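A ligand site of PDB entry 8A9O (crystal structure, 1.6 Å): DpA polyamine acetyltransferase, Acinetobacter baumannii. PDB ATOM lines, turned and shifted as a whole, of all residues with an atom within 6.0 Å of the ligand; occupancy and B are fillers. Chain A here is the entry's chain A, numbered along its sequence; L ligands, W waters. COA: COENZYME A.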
ATOM      1  N   TYR A  28      30.967   9.621   4.264  1.00  0.00           N
ATOM      2  CA  TYR A  28      30.068  10.419   3.462  1.00  0.00           C
ATOM      3  C   TYR A  28      30.865  11.221   2.423  1.00  0.00           C
ATOM      4  O   TYR A  28      30.480  11.287   1.264  1.00  0.00           O
ATOM      5  CB  TYR A  28      29.266  11.357   4.365  1.00  0.00           C
ATOM      6  CG  TYR A  28      28.441  12.389   3.630  1.00  0.00           C
ATOM      7  CD1 TYR A  28      27.284  12.012   2.938  1.00  0.00           C
ATOM      8  CD2 TYR A  28      28.802  13.718   3.627  1.00  0.00           C
ATOM      9  CE1 TYR A  28      26.498  12.965   2.302  1.00  0.00           C
ATOM     10  CE2 TYR A  28      28.026  14.674   2.978  1.00  0.00           C
ATOM     11  CZ  TYR A  28      26.879  14.291   2.314  1.00  0.00           C
ATOM     12  OH  TYR A  28      26.092  15.249   1.722  1.00  0.00           O
ATOM     13  N   PHE A  31      31.846   9.030  -0.321  1.00  0.00           N
ATOM     14  CA  PHE A  31      30.702   8.760  -1.235  1.00  0.00           C
ATOM     15  C   PHE A  31      30.676   9.793  -2.368  1.00  0.00           C
ATOM     16  O   PHE A  31      30.370   9.443  -3.509  1.00  0.00           O
ATOM     17  CB  PHE A  31      29.363   8.792  -0.462  1.00  0.00           C
ATOM     18  CG  PHE A  31      28.118   8.960  -1.303  1.00  0.00           C
ATOM     19  CD1 PHE A  31      27.567   7.885  -1.979  1.00  0.00           C
ATOM     20  CD2 PHE A  31      27.494  10.194  -1.424  1.00  0.00           C
ATOM     21  CE1 PHE A  31      26.431   8.043  -2.762  1.00  0.00           C
ATOM     22  CE2 PHE A  31      26.369  10.350  -2.229  1.00  0.00           C
ATOM     23  CZ  PHE A  31      25.847   9.264  -2.885  1.00  0.00           C
ATOM     24  N   TYR A  32      31.013  11.045  -2.062  1.00  0.00           N
ATOM     25  CA  TYR A  32      31.062  12.123  -3.031  1.00  0.00           C
ATOM     26  C   TYR A  32      32.416  12.282  -3.746  1.00  0.00           C
ATOM     27  O   TYR A  32      32.629  13.291  -4.417  1.00  0.00           O
ATOM     28  CB  TYR A  32      30.628  13.446  -2.383  1.00  0.00           C
ATOM     29  CG  TYR A  32      29.142  13.700  -2.398  1.00  0.00           C
ATOM     30  CD1 TYR A  32      28.474  13.932  -3.590  1.00  0.00           C
ATOM     31  CD2 TYR A  32      28.405  13.704  -1.230  1.00  0.00           C
ATOM     32  CE1 TYR A  32      27.099  14.190  -3.616  1.00  0.00           C
ATOM     33  CE2 TYR A  32      27.029  13.960  -1.241  1.00  0.00           C
ATOM     34  CZ  TYR A  32      26.391  14.200  -2.438  1.00  0.00           C
ATOM     35  OH  TYR A  32      25.026  14.423  -2.465  1.00  0.00           O
ATOM     36  N   ASP A  87      21.398  19.461   4.383  1.00  0.00           N
ATOM     37  CA  ASP A  87      22.616  19.490   3.578  1.00  0.00           C
ATOM     38  C   ASP A  87      23.251  18.152   3.351  1.00  0.00           C
ATOM     39  O   ASP A  87      23.683  17.846   2.233  1.00  0.00           O
ATOM     40  CB  ASP A  87      23.631  20.451   4.238  1.00  0.00           C
ATOM     41  CG  ASP A  87      24.600  21.108   3.250  1.00  0.00           C
ATOM     42  OD1 ASP A  87      24.371  20.993   2.010  1.00  0.00           O
ATOM     43  OD2 ASP A  87      25.566  21.742   3.712  1.00  0.00           O
ATOM     44  N   ASP A  88      23.363  17.356   4.408  1.00  0.00           N
ATOM     45  CA  ASP A  88      24.014  16.059   4.320  1.00  0.00           C
ATOM     46  C   ASP A  88      23.150  14.999   5.011  1.00  0.00           C
ATOM     47  O   ASP A  88      22.570  15.273   6.061  1.00  0.00           O
ATOM     48  CB  ASP A  88      25.366  16.116   5.046  1.00  0.00           C
ATOM     49  CG  ASP A  88      26.404  17.154   4.636  1.00  0.00           C
ATOM     50  OD1 ASP A  88      26.443  17.526   3.452  1.00  0.00           O
ATOM     51  OD2 ASP A  88      27.247  17.505   5.476  1.00  0.00           O
ATOM     52  N   VAL A  89      23.079  13.795   4.423  1.00  0.00           N
ATOM     53  CA  VAL A  89      22.301  12.682   4.937  1.00  0.00           C
ATOM     54  C   VAL A  89      23.184  11.444   4.678  1.00  0.00           C
ATOM     55  O   VAL A  89      23.595  11.247   3.527  1.00  0.00           O
ATOM     56  CB  VAL A  89      20.991  12.603   4.120  1.00  0.00           C
ATOM     57  CG1 VAL A  89      20.209  11.358   4.482  1.00  0.00           C
ATOM     58  CG2 VAL A  89      20.139  13.854   4.325  1.00  0.00           C
ATOM     59  N   TYR A  90      23.429  10.593   5.704  1.00  0.00           N
ATOM     60  CA  TYR A  90      24.270   9.412   5.479  1.00  0.00           C
ATOM     61  C   TYR A  90      24.019   8.334   6.524  1.00  0.00           C
ATOM     62  O   TYR A  90      23.925   8.631   7.719  1.00  0.00           O
ATOM     63  CB  TYR A  90      25.751   9.830   5.505  1.00  0.00           C
ATOM     64  CG  TYR A  90      26.702   8.674   5.280  1.00  0.00           C
ATOM     65  CD1 TYR A  90      26.952   8.203   3.999  1.00  0.00           C
ATOM     66  CD2 TYR A  90      27.281   8.018   6.347  1.00  0.00           C
ATOM     67  CE1 TYR A  90      27.771   7.099   3.783  1.00  0.00           C
ATOM     68  CE2 TYR A  90      28.091   6.888   6.148  1.00  0.00           C
ATOM     69  CZ  TYR A  90      28.330   6.440   4.864  1.00  0.00           C
ATOM     70  OH  TYR A  90      29.129   5.349   4.651  1.00  0.00           O
ATOM     71  N   VAL A  91      23.976   7.073   6.091  1.00  0.00           N
ATOM     72  CA  VAL A  91      23.871   5.904   6.975  1.00  0.00           C
ATOM     73  C   VAL A  91      25.002   4.947   6.558  1.00  0.00           C
ATOM     74  O   VAL A  91      25.234   4.749   5.352  1.00  0.00           O
ATOM     75  CB  VAL A  91      22.497   5.229   6.879  1.00  0.00           C
ATOM     76  CG1 VAL A  91      22.476   3.936   7.678  1.00  0.00           C
ATOM     77  CG2 VAL A  91      21.385   6.180   7.360  1.00  0.00           C
ATOM     78  N   THR A  92      25.790   4.453   7.542  1.00  0.00           N
ATOM     79  CA  THR A  92      26.907   3.569   7.222  1.00  0.00           C
ATOM     80  C   THR A  92      26.358   2.236   6.662  1.00  0.00           C
ATOM     81  O   THR A  92      25.308   1.774   7.084  1.00  0.00           O
ATOM     82  CB  THR A  92      27.832   3.444   8.450  1.00  0.00           C
ATOM     83  OG1 THR A  92      29.073   2.846   8.093  1.00  0.00           O
ATOM     84  CG2 THR A  92      27.191   2.696   9.590  1.00  0.00           C
ATOM     85  N   PHE A  95      24.457  -0.697   8.555  1.00  0.00           N
ATOM     86  CA  PHE A  95      23.137  -0.419   9.136  1.00  0.00           C
ATOM     87  C   PHE A  95      22.079   0.036   8.131  1.00  0.00           C
ATOM     88  O   PHE A  95      21.009   0.512   8.536  1.00  0.00           O
ATOM     89  CB  PHE A  95      23.278   0.643  10.244  1.00  0.00           C
ATOM     90  CG  PHE A  95      23.971   0.133  11.483  1.00  0.00           C
ATOM     91  CD1 PHE A  95      23.307  -0.671  12.386  1.00  0.00           C
ATOM     92  CD2 PHE A  95      25.289   0.460  11.739  1.00  0.00           C
ATOM     93  CE1 PHE A  95      23.962  -1.171  13.512  1.00  0.00           C
ATOM     94  CE2 PHE A  95      25.933   0.001  12.874  1.00  0.00           C
ATOM     95  CZ  PHE A  95      25.260  -0.828  13.757  1.00  0.00           C
ATOM     96  N   ARG A  96      22.353  -0.092   6.811  1.00  0.00           N
ATOM     97  CA  ARG A  96      21.385   0.379   5.811  1.00  0.00           C
ATOM     98  C   ARG A  96      20.146  -0.492   5.703  1.00  0.00           C
ATOM     99  O   ARG A  96      20.174  -1.694   6.031  1.00  0.00           O
ATOM    100  CB  ARG A  96      22.043   0.564   4.437  1.00  0.00           C
ATOM    101  CG  ARG A  96      22.999   1.742   4.433  1.00  0.00           C
ATOM    102  CD  ARG A  96      23.645   1.978   3.085  1.00  0.00           C
ATOM    103  NE  ARG A  96      24.619   3.054   3.219  1.00  0.00           N
ATOM    104  CZ  ARG A  96      25.513   3.400   2.319  1.00  0.00           C
ATOM    105  NH1 ARG A  96      25.594   2.746   1.161  1.00  0.00           N
ATOM    106  NH2 ARG A  96      26.356   4.404   2.565  1.00  0.00           N
ATOM    107  N   ARG A  97      19.052   0.137   5.251  1.00  0.00           N
ATOM    108  CA  ARG A  97      17.751  -0.500   5.027  1.00  0.00           C
ATOM    109  C   ARG A  97      17.102  -1.030   6.325  1.00  0.00           C
ATOM    110  O   ARG A  97      16.372  -2.023   6.337  1.00  0.00           O
ATOM    111  CB  ARG A  97      17.829  -1.595   3.960  1.00  0.00           C
ATOM    112  CG  ARG A  97      16.629  -1.558   3.026  1.00  0.00           C
ATOM    113  CD  ARG A  97      16.562  -0.295   2.160  1.00  0.00           C
ATOM    114  NE  ARG A  97      15.275  -0.210   1.489  1.00  0.00           N
ATOM    115  CZ  ARG A  97      15.033  -0.667   0.253  1.00  0.00           C
ATOM    116  NH1 ARG A  97      13.842  -0.535  -0.290  1.00  0.00           N
ATOM    117  NH2 ARG A  97      16.022  -1.225  -0.446  1.00  0.00           N
ATOM    118  N   GLN A  98      17.382  -0.344   7.417  1.00  0.00           N
ATOM    119  CA  GLN A  98      16.837  -0.608   8.739  1.00  0.00           C
ATOM    120  C   GLN A  98      15.970   0.581   9.219  1.00  0.00           C
ATOM    121  O   GLN A  98      15.504   0.545  10.340  1.00  0.00           O
ATOM    122  CB  GLN A  98      17.999  -0.802   9.724  1.00  0.00           C
ATOM    123  CG  GLN A  98      18.882  -2.043   9.443  1.00  0.00           C
ATOM    124  CD  GLN A  98      19.932  -2.247  10.526  1.00  0.00           C
ATOM    125  OE1 GLN A  98      19.974  -1.551  11.543  1.00  0.00           O
ATOM    126  NE2 GLN A  98      20.818  -3.195  10.332  1.00  0.00           N
ATOM    127  N   GLY A  99      15.835   1.660   8.420  1.00  0.00           N
ATOM    128  CA  GLY A  99      15.021   2.817   8.793  1.00  0.00           C
ATOM    129  C   GLY A  99      15.802   3.935   9.461  1.00  0.00           C
ATOM    130  O   GLY A  99      15.180   4.901   9.903  1.00  0.00           O
ATOM    131  N   SER A 100      17.152   3.861   9.534  1.00  0.00           N
ATOM    132  CA  SER A 100      17.925   4.953  10.161  1.00  0.00           C
ATOM    133  C   SER A 100      17.661   6.307   9.478  1.00  0.00           C
ATOM    134  O   SER A 100      17.374   7.280  10.153  1.00  0.00           O
ATOM    135  CB  SER A 100      19.430   4.663  10.211  1.00  0.00           C
ATOM    136  OG  SER A 100      19.727   3.513  10.990  1.00  0.00           O
ATOM    137  N   ALA A 101      17.761   6.365   8.117  1.00  0.00           N
ATOM    138  CA  ALA A 101      17.541   7.626   7.400  1.00  0.00           C
ATOM    139  C   ALA A 101      16.106   8.102   7.566  1.00  0.00           C
ATOM    140  O   ALA A 101      15.875   9.288   7.811  1.00  0.00           O
ATOM    141  CB  ALA A 101      17.898   7.470   5.923  1.00  0.00           C
ATOM    142  N   LYS A 102      15.137   7.174   7.516  1.00  0.00           N
ATOM    143  CA  LYS A 102      13.733   7.538   7.731  1.00  0.00           C
ATOM    144  C   LYS A 102      13.557   8.175   9.122  1.00  0.00           C
ATOM    145  O   LYS A 102      12.971   9.253   9.221  1.00  0.00           O
ATOM    146  CB  LYS A 102      12.842   6.281   7.609  1.00  0.00           C
ATOM    147  CG  LYS A 102      11.387   6.554   7.998  1.00  0.00           C
ATOM    148  CD  LYS A 102      10.534   5.307   7.966  1.00  0.00           C
ATOM    149  CE  LYS A 102       9.636   5.259   9.185  1.00  0.00           C
ATOM    150  NZ  LYS A 102       8.835   6.515   9.341  1.00  0.00           N
ATOM    151  N   GLN A 103      14.127   7.544  10.173  1.00  0.00           N
ATOM    152  CA  GLN A 103      14.023   8.076  11.550  1.00  0.00           C
ATOM    153  C   GLN A 103      14.741   9.432  11.698  1.00  0.00           C
ATOM    154  O   GLN A 103      14.226  10.340  12.346  1.00  0.00           O
ATOM    155  CB  GLN A 103      14.552   7.068  12.568  1.00  0.00           C
ATOM    156  CG  GLN A 103      13.668   5.803  12.582  1.00  0.00           C
ATOM    157  CD  GLN A 103      14.338   4.632  13.269  1.00  0.00           C
ATOM    158  OE1 GLN A 103      15.165   4.785  14.151  1.00  0.00           O
ATOM    159  NE2 GLN A 103      14.013   3.427  12.851  1.00  0.00           N
ATOM    160  N   GLU A 123      19.206  19.375  -2.001  1.00  0.00           N
ATOM    161  CA  GLU A 123      19.674  19.038  -3.335  1.00  0.00           C
ATOM    162  C   GLU A 123      20.372  17.672  -3.234  1.00  0.00           C
ATOM    163  O   GLU A 123      21.186  17.452  -2.341  1.00  0.00           O
ATOM    164  CB  GLU A 123      20.655  20.087  -3.896  1.00  0.00           C
ATOM    165  N   THR A 124      20.052  16.766  -4.151  1.00  0.00           N
ATOM    166  CA  THR A 124      20.692  15.454  -4.206  1.00  0.00           C
ATOM    167  C   THR A 124      21.081  15.190  -5.649  1.00  0.00           C
ATOM    168  O   THR A 124      20.499  15.792  -6.540  1.00  0.00           O
ATOM    169  CB  THR A 124      19.751  14.390  -3.634  1.00  0.00           C
ATOM    170  OG1 THR A 124      20.466  13.152  -3.519  1.00  0.00           O
ATOM    171  CG2 THR A 124      18.485  14.174  -4.480  1.00  0.00           C
ATOM    172  N   ASN A 128      21.045   9.786  -8.139  1.00  0.00           N
ATOM    173  CA  ASN A 128      20.971   9.072  -6.857  1.00  0.00           C
ATOM    174  C   ASN A 128      19.558   8.510  -6.682  1.00  0.00           C
ATOM    175  O   ASN A 128      18.729   9.085  -5.975  1.00  0.00           O
ATOM    176  CB  ASN A 128      21.344  10.034  -5.724  1.00  0.00           C
ATOM    177  CG  ASN A 128      21.579   9.324  -4.421  1.00  0.00           C
ATOM    178  OD1 ASN A 128      21.027   8.247  -4.170  1.00  0.00           O
ATOM    179  ND2 ASN A 128      22.366   9.953  -3.535  1.00  0.00           N
ATOM    180  N   HIS A 129      19.267   7.394  -7.333  1.00  0.00           N
ATOM    181  CA  HIS A 129      17.938   6.808  -7.270  1.00  0.00           C
ATOM    182  C   HIS A 129      17.513   6.392  -5.835  1.00  0.00           C
ATOM    183  O   HIS A 129      16.341   6.553  -5.494  1.00  0.00           O
ATOM    184  CB  HIS A 129      17.816   5.658  -8.274  1.00  0.00           C
ATOM    185  CG  HIS A 129      18.239   6.076  -9.651  1.00  0.00           C
ATOM    186  ND1 HIS A 129      17.544   7.046 -10.354  1.00  0.00           N
ATOM    187  CD2 HIS A 129      19.352   5.746 -10.349  1.00  0.00           C
ATOM    188  CE1 HIS A 129      18.226   7.234 -11.481  1.00  0.00           C
ATOM    189  NE2 HIS A 129      19.324   6.468 -11.522  1.00  0.00           N
ATOM    190  N   GLU A 130      18.454   5.926  -4.994  1.00  0.00           N
ATOM    191  CA  GLU A 130      18.130   5.547  -3.613  1.00  0.00           C
ATOM    192  C   GLU A 130      17.626   6.745  -2.806  1.00  0.00           C
ATOM    193  O   GLU A 130      16.591   6.667  -2.118  1.00  0.00           O
ATOM    194  CB  GLU A 130      19.368   4.941  -2.921  1.00  0.00           C
ATOM    195  CG  GLU A 130      19.851   3.647  -3.562  1.00  0.00           C
ATOM    196  CD  GLU A 130      20.629   3.757  -4.849  1.00  0.00           C
ATOM    197  OE1 GLU A 130      21.103   4.865  -5.181  1.00  0.00           O
ATOM    198  OE2 GLU A 130      20.757   2.728  -5.553  1.00  0.00           O
ATOM    199  N   SER A 131      18.334   7.890  -2.915  1.00  0.00           N
ATOM    200  CA  SER A 131      17.921   9.083  -2.173  1.00  0.00           C
ATOM    201  C   SER A 131      16.580   9.608  -2.675  1.00  0.00           C
ATOM    202  O   SER A 131      15.762  10.028  -1.857  1.00  0.00           O
ATOM    203  CB  SER A 131      18.999  10.162  -2.203  1.00  0.00           C
ATOM    204  OG  SER A 131      19.014  10.818  -3.462  1.00  0.00           O
ATOM    205  N   ARG A 133      14.001   7.920  -3.770  1.00  0.00           N
ATOM    206  CA  ARG A 133      12.975   7.053  -3.185  1.00  0.00           C
ATOM    207  C   ARG A 133      12.784   7.393  -1.700  1.00  0.00           C
ATOM    208  O   ARG A 133      11.650   7.497  -1.227  1.00  0.00           O
ATOM    209  CB  ARG A 133      13.381   5.586  -3.351  1.00  0.00           C
ATOM    210  N   LEU A 134      13.913   7.625  -0.976  1.00  0.00           N
ATOM    211  CA  LEU A 134      13.862   8.000   0.432  1.00  0.00           C
ATOM    212  C   LEU A 134      13.069   9.324   0.603  1.00  0.00           C
ATOM    213  O   LEU A 134      12.129   9.385   1.396  1.00  0.00           O
ATOM    214  CB  LEU A 134      15.317   8.168   0.960  1.00  0.00           C
ATOM    215  CG  LEU A 134      15.491   8.874   2.308  1.00  0.00           C
ATOM    216  CD1 LEU A 134      14.902   8.058   3.434  1.00  0.00           C
ATOM    217  CD2 LEU A 134      16.949   9.138   2.596  1.00  0.00           C
ATOM    218  N   TYR A 135      13.444  10.369  -0.144  1.00  0.00           N
ATOM    219  CA  TYR A 135      12.822  11.673   0.011  1.00  0.00           C
ATOM    220  C   TYR A 135      11.351  11.637  -0.364  1.00  0.00           C
ATOM    221  O   TYR A 135      10.522  12.184   0.372  1.00  0.00           O
ATOM    222  CB  TYR A 135      13.607  12.752  -0.742  1.00  0.00           C
ATOM    223  CG  TYR A 135      15.034  12.840  -0.247  1.00  0.00           C
ATOM    224  CD1 TYR A 135      15.324  12.793   1.110  1.00  0.00           C
ATOM    225  CD2 TYR A 135      16.080  13.061  -1.120  1.00  0.00           C
ATOM    226  CE1 TYR A 135      16.632  12.871   1.572  1.00  0.00           C
ATOM    227  CE2 TYR A 135      17.398  13.156  -0.669  1.00  0.00           C
ATOM    228  CZ  TYR A 135      17.669  13.067   0.678  1.00  0.00           C
ATOM    229  OH  TYR A 135      18.957  13.158   1.142  1.00  0.00           O
ATOM    230  N   LYS A 137       9.399   9.047  -0.091  1.00  0.00           N
ATOM    231  CA  LYS A 137       8.749   8.336   1.014  1.00  0.00           C
ATOM    232  C   LYS A 137       8.441   9.296   2.171  1.00  0.00           C
ATOM    233  O   LYS A 137       7.378   9.201   2.797  1.00  0.00           O
ATOM    234  CB  LYS A 137       9.624   7.152   1.492  1.00  0.00           C
ATOM    235  CG  LYS A 137       9.089   6.462   2.741  1.00  0.00           C
ATOM    236  CD  LYS A 137      10.011   5.384   3.272  1.00  0.00           C
ATOM    237  CE  LYS A 137       9.361   4.620   4.387  1.00  0.00           C
ATOM    238  NZ  LYS A 137       7.988   4.195   4.014  1.00  0.00           N
HETATM  239  N1A COA L   1      17.257   1.172  -2.876  1.00  0.00           N
HETATM  240  C2A COA L   1      16.048   1.706  -3.012  1.00  0.00           C
HETATM  241  N3A COA L   1      15.381   2.487  -2.170  1.00  0.00           N
HETATM  242  C4A COA L   1      16.091   2.716  -1.055  1.00  0.00           C
HETATM  243  C5A COA L   1      17.356   2.230  -0.771  1.00  0.00           C
HETATM  244  C6A COA L   1      17.956   1.411  -1.745  1.00  0.00           C
HETATM  245  N6A COA L   1      19.166   0.850  -1.616  1.00  0.00           N
HETATM  246  N7A COA L   1      17.788   2.677   0.467  1.00  0.00           N
HETATM  247  C8A COA L   1      16.791   3.410   0.901  1.00  0.00           C
HETATM  248  N9A COA L   1      15.730   3.482   0.021  1.00  0.00           N
HETATM  249  C1B COA L   1      14.479   4.199   0.230  1.00  0.00           C
HETATM  250  C2B COA L   1      13.236   3.305   0.291  1.00  0.00           C
HETATM  251  O2B COA L   1      12.138   4.111  -0.144  1.00  0.00           O
HETATM  252  C3B COA L   1      13.187   3.029   1.793  1.00  0.00           C
HETATM  253  O3B COA L   1      11.876   2.589   2.215  1.00  0.00           O
HETATM  254  P3B COA L   1      11.669   0.973   2.287  1.00  0.00           P
HETATM  255  O7A COA L   1      11.472   0.507   0.869  1.00  0.00           O
HETATM  256  O8A COA L   1      10.422   0.840   3.133  1.00  0.00           O
HETATM  257  O9A COA L   1      12.879   0.335   2.928  1.00  0.00           O
HETATM  258  C4B COA L   1      13.515   4.395   2.371  1.00  0.00           C
HETATM  259  O4B COA L   1      14.545   4.883   1.469  1.00  0.00           O
HETATM  260  C5B COA L   1      14.001   4.409   3.803  1.00  0.00           C
HETATM  261  O5B COA L   1      15.138   3.541   3.935  1.00  0.00           O
HETATM  262  P1A COA L   1      16.096   3.647   5.208  1.00  0.00           P
HETATM  263  O1A COA L   1      16.386   2.265   5.660  1.00  0.00           O
HETATM  264  O2A COA L   1      15.602   4.626   6.191  1.00  0.00           O
HETATM  265  O3A COA L   1      17.413   4.174   4.458  1.00  0.00           O
HETATM  266  P2A COA L   1      18.917   3.953   4.951  1.00  0.00           P
HETATM  267  O4A COA L   1      18.929   4.142   6.420  1.00  0.00           O
HETATM  268  O5A COA L   1      19.448   2.686   4.389  1.00  0.00           O
HETATM  269  O6A COA L   1      19.664   5.214   4.353  1.00  0.00           O
HETATM  270  CBP COA L   1      20.613   6.397   2.460  1.00  0.00           C
HETATM  271  CCP COA L   1      19.438   5.584   2.982  1.00  0.00           C
HETATM  272  CDP COA L   1      20.274   6.905   1.045  1.00  0.00           C
HETATM  273  CEP COA L   1      20.836   7.596   3.390  1.00  0.00           C
HETATM  274  CAP COA L   1      21.884   5.499   2.415  1.00  0.00           C
HETATM  275  OAP COA L   1      21.749   4.471   1.416  1.00  0.00           O
HETATM  276  C9P COA L   1      23.203   6.254   2.208  1.00  0.00           C
HETATM  277  O9P COA L   1      23.821   6.725   3.164  1.00  0.00           O
HETATM  278  N8P COA L   1      23.650   6.356   0.949  1.00  0.00           N
HETATM  279  C7P COA L   1      24.904   7.024   0.606  1.00  0.00           C
HETATM  280  C6P COA L   1      24.857   8.525   0.823  1.00  0.00           C
HETATM  281  C5P COA L   1      23.638   9.147   0.192  1.00  0.00           C
HETATM  282  O5P COA L   1      23.221   8.786  -0.910  1.00  0.00           O
HETATM  283  N4P COA L   1      23.001  10.036   0.943  1.00  0.00           N
HETATM  284  C3P COA L   1      21.894  10.831   0.455  1.00  0.00           C
HETATM  285  C2P COA L   1      22.438  11.958  -0.314  1.00  0.00           C
HETATM  286  S1P COA L   1      23.278  13.102   0.803  1.00  0.00           S
HETATM  287  O   HOH W   1      23.625   4.400  -1.767  1.00  0.00           O
HETATM  288  O   HOH W   2      22.918   6.606  -2.653  1.00  0.00           O
HETATM  289  O   HOH W   3      20.215   2.302   1.862  1.00  0.00           O
HETATM  290  O   HOH W   4      17.553  -0.848  -4.710  1.00  0.00           O
HETATM  291  O   HOH W   5       8.442  -0.717   2.794  1.00  0.00           O
HETATM  292  O   HOH W   6      14.144   0.731   5.379  1.00  0.00           O
HETATM  293  O   HOH W   7      21.099  -0.035   0.845  1.00  0.00           O
HETATM  294  O   HOH W   8      18.926   2.026   8.087  1.00  0.00           O
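Water W2 lies within hydrogen-bond range of an oxygen (O5P) of the ligand and the side-chain amide oxygen (OD1) of Asn 128.
O of Gly 99 sits close to NE2 of Gln 103, at 3.5 Å. NE of Arg 96 lies within hydrogen-bond range of O of Val 91 (2.8 Å). The backbone NH of Ser 131 is in hydrogen-bond range of the side-chain amide oxygen of Asn 128 (3.0 Å). The side-chain hydroxyl (OH) of Tyr 28 is in hydrogen-bond range of the side-chain carboxylate (OD1) of Asp 88 (2.9 Å). The side-chain hydroxyl (OG1) of Thr 124 is in hydrogen-bond range of the side-chain hydroxyl (OG) of Ser 131.
Residues that only touch the ligand: Phe 31 (3.3 Å), Leu 134 (3.4 Å), Glu 130 (3.4 Å), Lys 137 (3.5 Å), Tyr 90 (3.6 Å), Arg 133 (3.6 Å), Ser 100 (3.6 Å), Tyr 135 (3.8 Å), Tyr 32 (3.9 Å), Thr 124 (3.9 Å) and Ser 131 (3.99 Å). Hydrophobic or aromatic side chains that line the ligand: Tyr 28, Phe 31, Val 89, Tyr 90, Val 91, Ala 101 and Leu 134. Of the 28 residues printed, 21 come within 4 Å of the ligand. The nearest printed residue that does not touch the ligand is Asp 88 (4.6 Å).
N of Arg 97 is in hydrogen-bond range of O5A of the ligand (2.7 Å). NH1 of Arg 97 lies within salt-bridge range of O7A of the ligand (2.8 Å). O1A of the ligand is in hydrogen-bond range of N of Gly 99, 2.9 Å away. The backbone NH (N) of Lys 102 is in hydrogen-bond range of an oxygen (O2A) of the ligand. N of Val 89 lies close to S1P of the ligand (3.7 Å). O of Val 89 sits at hydrogen-bond distance from N4P of the ligand, at 2.9 Å. An oxygen (O9P) of the ligand lies within hydrogen-bond range of the backbone NH (N) of Val 91 (3.0 Å). ND2 of Asn 128 lies within hydrogen-bond range of O5P of the ligand (3.0 Å). O4A of the ligand sits at hydrogen-bond distance from N of Ala 101, at 3.0 Å. An oxygen (O1A) of the ligand lies within hydrogen-bond range of the backbone NH (N) of Gln 98 (3.3 Å). O9P of the ligand sits at hydrogen-bond distance from NH2 of Arg 96 (3.5 Å). S1P of the ligand lies close to OH of Tyr 28 (3.7 Å).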
